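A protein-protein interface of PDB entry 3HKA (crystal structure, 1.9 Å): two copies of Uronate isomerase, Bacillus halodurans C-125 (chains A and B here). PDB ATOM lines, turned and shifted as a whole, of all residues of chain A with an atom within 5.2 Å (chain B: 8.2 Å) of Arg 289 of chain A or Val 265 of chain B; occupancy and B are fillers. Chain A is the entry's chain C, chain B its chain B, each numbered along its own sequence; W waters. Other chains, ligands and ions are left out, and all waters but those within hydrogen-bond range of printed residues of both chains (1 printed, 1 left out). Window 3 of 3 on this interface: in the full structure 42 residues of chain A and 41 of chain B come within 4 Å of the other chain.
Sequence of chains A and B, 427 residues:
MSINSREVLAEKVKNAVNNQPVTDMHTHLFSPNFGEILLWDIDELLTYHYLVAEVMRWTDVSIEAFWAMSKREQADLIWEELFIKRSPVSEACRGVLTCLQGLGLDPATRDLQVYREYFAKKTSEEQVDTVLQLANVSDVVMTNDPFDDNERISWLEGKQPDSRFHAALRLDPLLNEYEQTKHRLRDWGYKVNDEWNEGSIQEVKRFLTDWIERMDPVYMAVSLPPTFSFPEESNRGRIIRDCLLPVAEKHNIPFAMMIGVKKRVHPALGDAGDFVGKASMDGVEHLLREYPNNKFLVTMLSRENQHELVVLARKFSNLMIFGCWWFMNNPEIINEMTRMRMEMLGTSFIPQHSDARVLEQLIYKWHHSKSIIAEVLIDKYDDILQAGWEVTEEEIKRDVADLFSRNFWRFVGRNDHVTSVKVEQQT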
ATOM      1  N   VAL A 284     -22.764 -29.053  30.424  1.00  0.00           N
ATOM      2  CA  VAL A 284     -22.203 -29.620  29.208  1.00  0.00           C
ATOM      3  C   VAL A 284     -21.706 -28.482  28.319  1.00  0.00           C
ATOM      4  O   VAL A 284     -20.627 -28.566  27.737  1.00  0.00           O
ATOM      5  CB  VAL A 284     -23.257 -30.465  28.448  1.00  0.00           C
ATOM      6  CG1 VAL A 284     -22.616 -31.145  27.250  1.00  0.00           C
ATOM      7  CG2 VAL A 284     -23.861 -31.511  29.395  1.00  0.00           C
ATOM      8  N   GLU A 285     -22.494 -27.413  28.229  1.00  0.00           N
ATOM      9  CA  GLU A 285     -22.134 -26.244  27.419  1.00  0.00           C
ATOM     10  C   GLU A 285     -20.800 -25.683  27.932  1.00  0.00           C
ATOM     11  O   GLU A 285     -19.877 -25.409  27.158  1.00  0.00           O
ATOM     12  CB  GLU A 285     -23.223 -25.168  27.546  1.00  0.00           C
ATOM     13  CG  GLU A 285     -22.952 -23.870  26.793  1.00  0.00           C
ATOM     14  CD  GLU A 285     -23.829 -22.730  27.291  1.00  0.00           C
ATOM     15  OE1 GLU A 285     -25.023 -22.976  27.565  1.00  0.00           O
ATOM     16  OE2 GLU A 285     -23.333 -21.590  27.405  1.00  0.00           O
ATOM     17  N   HIS A 286     -20.711 -25.523  29.247  1.00  0.00           N
ATOM     18  CA  HIS A 286     -19.501 -24.996  29.863  1.00  0.00           C
ATOM     19  C   HIS A 286     -18.283 -25.846  29.520  1.00  0.00           C
ATOM     20  O   HIS A 286     -17.260 -25.330  29.064  1.00  0.00           O
ATOM     21  CB  HIS A 286     -19.654 -24.944  31.383  1.00  0.00           C
ATOM     22  CG  HIS A 286     -18.448 -24.406  32.087  1.00  0.00           C
ATOM     23  ND1 HIS A 286     -18.345 -23.094  32.492  1.00  0.00           N
ATOM     24  CD2 HIS A 286     -17.278 -25.000  32.427  1.00  0.00           C
ATOM     25  CE1 HIS A 286     -17.165 -22.901  33.057  1.00  0.00           C
ATOM     26  NE2 HIS A 286     -16.499 -24.042  33.029  1.00  0.00           N
ATOM     27  N   LEU A 287     -18.396 -27.152  29.754  1.00  0.00           N
ATOM     28  CA  LEU A 287     -17.305 -28.074  29.484  1.00  0.00           C
ATOM     29  C   LEU A 287     -16.819 -27.986  28.044  1.00  0.00           C
ATOM     30  O   LEU A 287     -15.614 -27.887  27.794  1.00  0.00           O
ATOM     31  CB  LEU A 287     -17.744 -29.505  29.809  1.00  0.00           C
ATOM     32  CG  LEU A 287     -17.799 -29.813  31.313  1.00  0.00           C
ATOM     33  CD1 LEU A 287     -18.585 -31.095  31.553  1.00  0.00           C
ATOM     34  CD2 LEU A 287     -16.375 -29.941  31.866  1.00  0.00           C
ATOM     35  N   LEU A 288     -17.757 -28.020  27.102  1.00  0.00           N
ATOM     36  CA  LEU A 288     -17.424 -27.941  25.683  1.00  0.00           C
ATOM     37  C   LEU A 288     -16.713 -26.641  25.326  1.00  0.00           C
ATOM     38  O   LEU A 288     -15.701 -26.649  24.613  1.00  0.00           O
ATOM     39  CB  LEU A 288     -18.692 -28.070  24.839  1.00  0.00           C
ATOM     40  CG  LEU A 288     -19.350 -29.446  24.880  1.00  0.00           C
ATOM     41  CD1 LEU A 288     -20.718 -29.389  24.210  1.00  0.00           C
ATOM     42  CD2 LEU A 288     -18.439 -30.462  24.167  1.00  0.00           C
ATOM     43  N   ARG A 289     -17.241 -25.523  25.815  1.00  0.00           N
ATOM     44  CA  ARG A 289     -16.643 -24.227  25.515  1.00  0.00           C
ATOM     45  C   ARG A 289     -15.301 -23.968  26.188  1.00  0.00           C
ATOM     46  O   ARG A 289     -14.362 -23.508  25.545  1.00  0.00           O
ATOM     47  CB  ARG A 289     -17.598 -23.084  25.891  1.00  0.00           C
ATOM     48  CG  ARG A 289     -16.975 -21.691  25.681  1.00  0.00           C
ATOM     49  CD  ARG A 289     -17.920 -20.551  26.063  1.00  0.00           C
ATOM     50  NE  ARG A 289     -18.496 -20.757  27.386  1.00  0.00           N
ATOM     51  CZ  ARG A 289     -19.770 -21.078  27.602  1.00  0.00           C
ATOM     52  NH1 ARG A 289     -20.606 -21.221  26.581  1.00  0.00           N
ATOM     53  NH2 ARG A 289     -20.205 -21.268  28.841  1.00  0.00           N
ATOM     54  N   GLU A 290     -15.212 -24.265  27.477  1.00  0.00           N
ATOM     55  CA  GLU A 290     -13.998 -23.995  28.231  1.00  0.00           C
ATOM     56  C   GLU A 290     -12.879 -25.022  28.099  1.00  0.00           C
ATOM     57  O   GLU A 290     -11.742 -24.744  28.465  1.00  0.00           O
ATOM     58  CB  GLU A 290     -14.344 -23.795  29.706  1.00  0.00           C
ATOM     59  CG  GLU A 290     -15.434 -22.747  29.967  1.00  0.00           C
ATOM     60  CD  GLU A 290     -15.134 -21.383  29.349  1.00  0.00           C
ATOM     61  OE1 GLU A 290     -13.947 -21.048  29.164  1.00  0.00           O
ATOM     62  OE2 GLU A 290     -16.094 -20.632  29.067  1.00  0.00           O
ATOM     63  N   TYR A 291     -13.197 -26.205  27.586  1.00  0.00           N
ATOM     64  CA  TYR A 291     -12.191 -27.245  27.399  1.00  0.00           C
ATOM     65  C   TYR A 291     -12.167 -27.680  25.942  1.00  0.00           C
ATOM     66  O   TYR A 291     -12.421 -28.844  25.614  1.00  0.00           O
ATOM     67  CB  TYR A 291     -12.499 -28.423  28.312  1.00  0.00           C
ATOM     68  CG  TYR A 291     -12.291 -28.075  29.764  1.00  0.00           C
ATOM     69  CD1 TYR A 291     -11.049 -28.252  30.367  1.00  0.00           C
ATOM     70  CD2 TYR A 291     -13.328 -27.546  30.529  1.00  0.00           C
ATOM     71  CE1 TYR A 291     -10.840 -27.916  31.700  1.00  0.00           C
ATOM     72  CE2 TYR A 291     -13.134 -27.203  31.871  1.00  0.00           C
ATOM     73  CZ  TYR A 291     -11.890 -27.395  32.445  1.00  0.00           C
ATOM     74  OH  TYR A 291     -11.693 -27.091  33.770  1.00  0.00           O
ATOM     75  N   PRO A 292     -11.841 -26.739  25.046  1.00  0.00           N
ATOM     76  CA  PRO A 292     -11.779 -26.988  23.605  1.00  0.00           C
ATOM     77  C   PRO A 292     -10.819 -28.107  23.209  1.00  0.00           C
ATOM     78  O   PRO A 292     -10.959 -28.693  22.139  1.00  0.00           O
ATOM     79  CB  PRO A 292     -11.363 -25.630  23.042  1.00  0.00           C
ATOM     80  CG  PRO A 292     -10.486 -25.078  24.132  1.00  0.00           C
ATOM     81  CD  PRO A 292     -11.276 -25.416  25.377  1.00  0.00           C
ATOM     82  N   LYS A 315     -23.206 -26.419  17.906  1.00  0.00           N
ATOM     83  CA  LYS A 315     -22.302 -25.379  18.395  1.00  0.00           C
ATOM     84  C   LYS A 315     -20.855 -25.824  18.599  1.00  0.00           C
ATOM     85  O   LYS A 315     -19.927 -25.048  18.378  1.00  0.00           O
ATOM     86  CB  LYS A 315     -22.787 -24.820  19.741  1.00  0.00           C
ATOM     87  CG  LYS A 315     -24.231 -24.326  19.805  1.00  0.00           C
ATOM     88  CD  LYS A 315     -24.491 -23.143  18.891  1.00  0.00           C
ATOM     89  CE  LYS A 315     -25.186 -23.574  17.608  1.00  0.00           C
ATOM     90  NZ  LYS A 315     -25.710 -22.388  16.874  1.00  0.00           N
ATOM     91  N   PHE A 316     -20.663 -27.068  19.022  1.00  0.00           N
ATOM     92  CA  PHE A 316     -19.322 -27.550  19.352  1.00  0.00           C
ATOM     93  C   PHE A 316     -18.881 -28.833  18.676  1.00  0.00           C
ATOM     94  O   PHE A 316     -19.510 -29.880  18.833  1.00  0.00           O
ATOM     95  CB  PHE A 316     -19.232 -27.726  20.872  1.00  0.00           C
ATOM     96  CG  PHE A 316     -19.473 -26.457  21.642  1.00  0.00           C
ATOM     97  CD1 PHE A 316     -18.502 -25.461  21.682  1.00  0.00           C
ATOM     98  CD2 PHE A 316     -20.682 -26.248  22.305  1.00  0.00           C
ATOM     99  CE1 PHE A 316     -18.728 -24.270  22.368  1.00  0.00           C
ATOM    100  CE2 PHE A 316     -20.924 -25.056  22.999  1.00  0.00           C
ATOM    101  CZ  PHE A 316     -19.944 -24.065  23.031  1.00  0.00           C
ATOM    102  N   ASN A 318     -16.267 -30.477  19.420  1.00  0.00           N
ATOM    103  CA  ASN A 318     -15.630 -31.389  20.367  1.00  0.00           C
ATOM    104  C   ASN A 318     -16.706 -32.167  21.135  1.00  0.00           C
ATOM    105  O   ASN A 318     -16.438 -32.838  22.132  1.00  0.00           O
ATOM    106  CB  ASN A 318     -14.657 -30.644  21.307  1.00  0.00           C
ATOM    107  CG  ASN A 318     -15.318 -29.538  22.122  1.00  0.00           C
ATOM    108  OD1 ASN A 318     -16.273 -28.898  21.680  1.00  0.00           O
ATOM    109  ND2 ASN A 318     -14.778 -29.288  23.320  1.00  0.00           N
ATOM    110  N   VAL B 261     -33.652 -17.737  22.780  1.00  0.00           N
ATOM    111  CA  VAL B 261     -32.290 -17.765  22.268  1.00  0.00           C
ATOM    112  C   VAL B 261     -31.233 -17.371  23.298  1.00  0.00           C
ATOM    113  O   VAL B 261     -31.360 -16.361  23.983  1.00  0.00           O
ATOM    114  CB  VAL B 261     -32.155 -16.872  20.990  1.00  0.00           C
ATOM    115  CG1 VAL B 261     -32.477 -15.410  21.317  1.00  0.00           C
ATOM    116  CG2 VAL B 261     -30.750 -17.010  20.405  1.00  0.00           C
ATOM    117  N   LYS B 262     -30.206 -18.207  23.420  1.00  0.00           N
ATOM    118  CA  LYS B 262     -29.101 -17.943  24.336  1.00  0.00           C
ATOM    119  C   LYS B 262     -27.960 -17.500  23.424  1.00  0.00           C
ATOM    120  O   LYS B 262     -27.285 -18.320  22.806  1.00  0.00           O
ATOM    121  CB  LYS B 262     -28.723 -19.210  25.110  1.00  0.00           C
ATOM    122  CG  LYS B 262     -27.705 -18.964  26.218  1.00  0.00           C
ATOM    123  CD  LYS B 262     -27.546 -20.169  27.151  1.00  0.00           C
ATOM    124  CE  LYS B 262     -26.470 -19.900  28.206  1.00  0.00           C
ATOM    125  NZ  LYS B 262     -26.256 -21.046  29.137  1.00  0.00           N
ATOM    126  N   LYS B 263     -27.762 -16.191  23.341  1.00  0.00           N
ATOM    127  CA  LYS B 263     -26.749 -15.617  22.466  1.00  0.00           C
ATOM    128  C   LYS B 263     -25.287 -15.933  22.753  1.00  0.00           C
ATOM    129  O   LYS B 263     -24.844 -15.967  23.902  1.00  0.00           O
ATOM    130  CB  LYS B 263     -26.913 -14.091  22.417  1.00  0.00           C
ATOM    131  CG  LYS B 263     -28.308 -13.613  22.049  1.00  0.00           C
ATOM    132  CD  LYS B 263     -28.693 -13.998  20.625  1.00  0.00           C
ATOM    133  CE  LYS B 263     -27.887 -13.226  19.580  1.00  0.00           C
ATOM    134  NZ  LYS B 263     -28.329 -13.561  18.193  1.00  0.00           N
ATOM    135  N   ARG B 264     -24.550 -16.164  21.672  1.00  0.00           N
ATOM    136  CA  ARG B 264     -23.116 -16.414  21.718  1.00  0.00           C
ATOM    137  C   ARG B 264     -22.560 -17.416  22.729  1.00  0.00           C
ATOM    138  O   ARG B 264     -21.671 -17.063  23.504  1.00  0.00           O
ATOM    139  CB  ARG B 264     -22.391 -15.077  21.920  1.00  0.00           C
ATOM    140  CG  ARG B 264     -22.727 -14.009  20.880  1.00  0.00           C
ATOM    141  CD  ARG B 264     -22.107 -12.663  21.267  1.00  0.00           C
ATOM    142  NE  ARG B 264     -22.612 -12.176  22.553  1.00  0.00           N
ATOM    143  CZ  ARG B 264     -23.783 -11.568  22.723  1.00  0.00           C
ATOM    144  NH1 ARG B 264     -24.587 -11.355  21.685  1.00  0.00           N
ATOM    145  NH2 ARG B 264     -24.163 -11.189  23.937  1.00  0.00           N
ATOM    146  N   VAL B 265     -23.056 -18.652  22.738  1.00  0.00           N
ATOM    147  CA  VAL B 265     -22.500 -19.629  23.661  1.00  0.00           C
ATOM    148  C   VAL B 265     -21.153 -20.061  23.090  1.00  0.00           C
ATOM    149  O   VAL B 265     -20.321 -20.639  23.791  1.00  0.00           O
ATOM    150  CB  VAL B 265     -23.428 -20.858  23.864  1.00  0.00           C
ATOM    151  CG1 VAL B 265     -24.759 -20.396  24.449  1.00  0.00           C
ATOM    152  CG2 VAL B 265     -23.623 -21.602  22.567  1.00  0.00           C
ATOM    153  N   HIS B 266     -20.952 -19.774  21.805  1.00  0.00           N
ATOM    154  CA  HIS B 266     -19.690 -20.063  21.121  1.00  0.00           C
ATOM    155  C   HIS B 266     -19.384 -18.819  20.285  1.00  0.00           C
ATOM    156  O   HIS B 266     -19.678 -18.771  19.088  1.00  0.00           O
ATOM    157  CB  HIS B 266     -19.807 -21.293  20.218  1.00  0.00           C
ATOM    158  CG  HIS B 266     -18.492 -21.773  19.687  1.00  0.00           C
ATOM    159  ND1 HIS B 266     -18.336 -23.001  19.078  1.00  0.00           N
ATOM    160  CD2 HIS B 266     -17.269 -21.189  19.670  1.00  0.00           C
ATOM    161  CE1 HIS B 266     -17.076 -23.152  18.711  1.00  0.00           C
ATOM    162  NE2 HIS B 266     -16.407 -22.068  19.059  1.00  0.00           N
ATOM    163  N   PRO B 267     -18.789 -17.792  20.921  1.00  0.00           N
ATOM    164  CA  PRO B 267     -18.423 -16.508  20.311  1.00  0.00           C
ATOM    165  C   PRO B 267     -17.741 -16.572  18.948  1.00  0.00           C
ATOM    166  O   PRO B 267     -18.142 -15.872  18.016  1.00  0.00           O
ATOM    167  CB  PRO B 267     -17.528 -15.861  21.373  1.00  0.00           C
ATOM    168  CG  PRO B 267     -18.092 -16.403  22.654  1.00  0.00           C
ATOM    169  CD  PRO B 267     -18.301 -17.863  22.311  1.00  0.00           C
ATOM    170  N   ALA B 268     -16.716 -17.408  18.833  1.00  0.00           N
ATOM    171  CA  ALA B 268     -15.965 -17.540  17.587  1.00  0.00           C
ATOM    172  C   ALA B 268     -16.807 -17.905  16.366  1.00  0.00           C
ATOM    173  O   ALA B 268     -16.401 -17.640  15.230  1.00  0.00           O
ATOM    174  CB  ALA B 268     -14.846 -18.560  17.764  1.00  0.00           C
ATOM    175  N   LEU B 269     -17.968 -18.515  16.586  1.00  0.00           N
ATOM    176  CA  LEU B 269     -18.832 -18.903  15.473  1.00  0.00           C
ATOM    177  C   LEU B 269     -19.706 -17.774  14.949  1.00  0.00           C
ATOM    178  O   LEU B 269     -20.423 -17.953  13.970  1.00  0.00           O
ATOM    179  CB  LEU B 269     -19.738 -20.080  15.861  1.00  0.00           C
ATOM    180  CG  LEU B 269     -19.135 -21.485  15.939  1.00  0.00           C
ATOM    181  CD1 LEU B 269     -20.242 -22.475  16.284  1.00  0.00           C
ATOM    182  CD2 LEU B 269     -18.493 -21.863  14.610  1.00  0.00           C
ATOM    183  N   GLY B 270     -19.660 -16.619  15.601  1.00  0.00           N
ATOM    184  CA  GLY B 270     -20.471 -15.500  15.155  1.00  0.00           C
ATOM    185  C   GLY B 270     -21.961 -15.792  15.170  1.00  0.00           C
ATOM    186  O   GLY B 270     -22.496 -16.280  16.170  1.00  0.00           O
ATOM    187  N   ALA B 272     -23.459 -18.083  14.034  1.00  0.00           N
ATOM    188  CA  ALA B 272     -23.698 -19.515  14.170  1.00  0.00           C
ATOM    189  C   ALA B 272     -23.426 -20.026  15.583  1.00  0.00           C
ATOM    190  O   ALA B 272     -23.486 -21.231  15.830  1.00  0.00           O
ATOM    191  CB  ALA B 272     -22.832 -20.278  13.176  1.00  0.00           C
ATOM    192  N   GLY B 273     -23.139 -19.116  16.509  1.00  0.00           N
ATOM    193  CA  GLY B 273     -22.835 -19.530  17.868  1.00  0.00           C
ATOM    194  C   GLY B 273     -23.923 -19.355  18.913  1.00  0.00           C
ATOM    195  O   GLY B 273     -23.614 -19.318  20.105  1.00  0.00           O
ATOM    196  N   ASP B 274     -25.182 -19.250  18.488  1.00  0.00           N
ATOM    197  CA  ASP B 274     -26.281 -19.077  19.438  1.00  0.00           C
ATOM    198  C   ASP B 274     -26.912 -20.423  19.798  1.00  0.00           C
ATOM    199  O   ASP B 274     -27.002 -21.324  18.961  1.00  0.00           O
ATOM    200  CB  ASP B 274     -27.346 -18.126  18.873  1.00  0.00           C
ATOM    201  CG  ASP B 274     -26.810 -16.728  18.618  1.00  0.00           C
ATOM    202  OD1 ASP B 274     -25.809 -16.330  19.261  1.00  0.00           O
ATOM    203  OD2 ASP B 274     -27.408 -16.015  17.783  1.00  0.00           O
ATOM    204  N   PHE B 275     -27.355 -20.548  21.048  1.00  0.00           N
ATOM    205  CA  PHE B 275     -27.938 -21.793  21.559  1.00  0.00           C
ATOM    206  C   PHE B 275     -29.410 -21.584  21.943  1.00  0.00           C
ATOM    207  O   PHE B 275     -29.978 -20.522  21.675  1.00  0.00           O
ATOM    208  CB  PHE B 275     -27.079 -22.258  22.758  1.00  0.00           C
ATOM    209  CG  PHE B 275     -27.429 -23.625  23.309  1.00  0.00           C
ATOM    210  CD1 PHE B 275     -27.790 -24.679  22.469  1.00  0.00           C
ATOM    211  CD2 PHE B 275     -27.348 -23.864  24.679  1.00  0.00           C
ATOM    212  CE1 PHE B 275     -28.066 -25.949  22.991  1.00  0.00           C
ATOM    213  CE2 PHE B 275     -27.621 -25.129  25.212  1.00  0.00           C
ATOM    214  CZ  PHE B 275     -27.982 -26.175  24.367  1.00  0.00           C
ATOM    215  N   VAL B 276     -30.026 -22.591  22.558  1.00  0.00           N
ATOM    216  CA  VAL B 276     -31.434 -22.521  22.943  1.00  0.00           C
ATOM    217  C   VAL B 276     -31.690 -22.991  24.374  1.00  0.00           C
ATOM    218  O   VAL B 276     -30.892 -23.722  24.955  1.00  0.00           O
ATOM    219  CB  VAL B 276     -32.301 -23.397  21.991  1.00  0.00           C
ATOM    220  CG1 VAL B 276     -31.846 -24.859  22.080  1.00  0.00           C
ATOM    221  CG2 VAL B 276     -33.784 -23.279  22.346  1.00  0.00           C
HETATM  222  O   HOH W   1     -27.221 -24.167  28.516  1.00  0.00           O
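NZ of Lys 315 of chain A is in hydrogen-bond range of O of Asp 274 of chain B (2.7 Å). The guanidinium group (NH1) of Arg 289 of chain A lies within hydrogen-bond range of the backbone carbonyl oxygen (O) of Val 265 of chain B (2.9 Å). OE1 of Glu 285 of chain A is in salt-bridge range of NZ of Lys 262 of chain B (2.8 Å). The backbone carbonyl oxygen (O) of Ala 272 of chain B is in hydrogen-bond range of the side-chain amino group (NZ) of Lys 315 of chain A, 2.7 Å away. A ring nitrogen (ND1) of His 266 of chain B lies within hydrogen-bond range of the backbone carbonyl oxygen of Lys 315 of chain A.
Water W1 bridges the side-chain carboxylate of Glu 285 of chain A (2.7 Å) and the side-chain amino group of Lys 262 of chain B (3.3 Å).
The backbone carbonyl oxygen of Gly 273 of chain B lies within hydrogen-bond range of the backbone NH of Val 265 of chain B (2.8 Å). The guanidinium group (NH1) of Arg 289 of chain A is in salt-bridge range of the side-chain carboxylate (OE2) of Glu 285 of chain A. N of His 266 of chain B is in hydrogen-bond range of O of Gly 273 of chain B (3.2 Å). OD1 of Asp 274 of chain B sits at hydrogen-bond distance from N of Arg 264 of chain B (2.7 Å). The backbone NH of Phe 275 of chain B is in hydrogen-bond range of the backbone carbonyl oxygen of Lys 262 of chain B (2.8 Å). NZ of Lys 263 of chain B is in salt-bridge range of OD2 of Asp 274 of chain B, at 2.7 Å.
Of the 12 printed residues of chain A, 4 touch a printed residue of chain B. Hydrophobic or aromatic side chains of chain A within 4 Å of the printed part of chain B: Phe 316. Of the 15 printed residues of chain B, 8 touch a printed residue of chain A. Among the printed residues, Asp or Glu carboxylates within 4 Å of a Lys or Arg side-chain nitrogen of the other chain: Glu 285 of chain A with Lys 262 of chain B.
Of the printed residues of chain A, Gly 273 of chain B touches Lys 315 (3.8 Å). Of the printed residues of chain A, Phe 275 of chain B touches Glu 285 (3.8 Å). Of the printed residues of chain A, Leu 269 of chain B touches Lys 315. Of the printed residues of chain A, Ala 272 of chain B touches Lys 315. Of the printed residues of chain B, Phe 316 of chain A touches Val 265 and His 266.
No position is printed for both chains. Of the 12 pairs that touch across the chains among the printed residues, none has its exchanged pair printed and touching as well.
Among the printed residues, pairs that only touch across the chains: Glu 285 of chain A with Val 265 of chain B, Glu 285 of chain A with Phe 275 of chain B, Lys 315 of chain A with Val 265 of chain B, Lys 315 of chain A with Leu 269 of chain B, Lys 315 of chain A with Gly 273 of chain B, Phe 316 of chain A with Val 265 of chain B and Phe 316 of chain A with His 266 of chain B.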
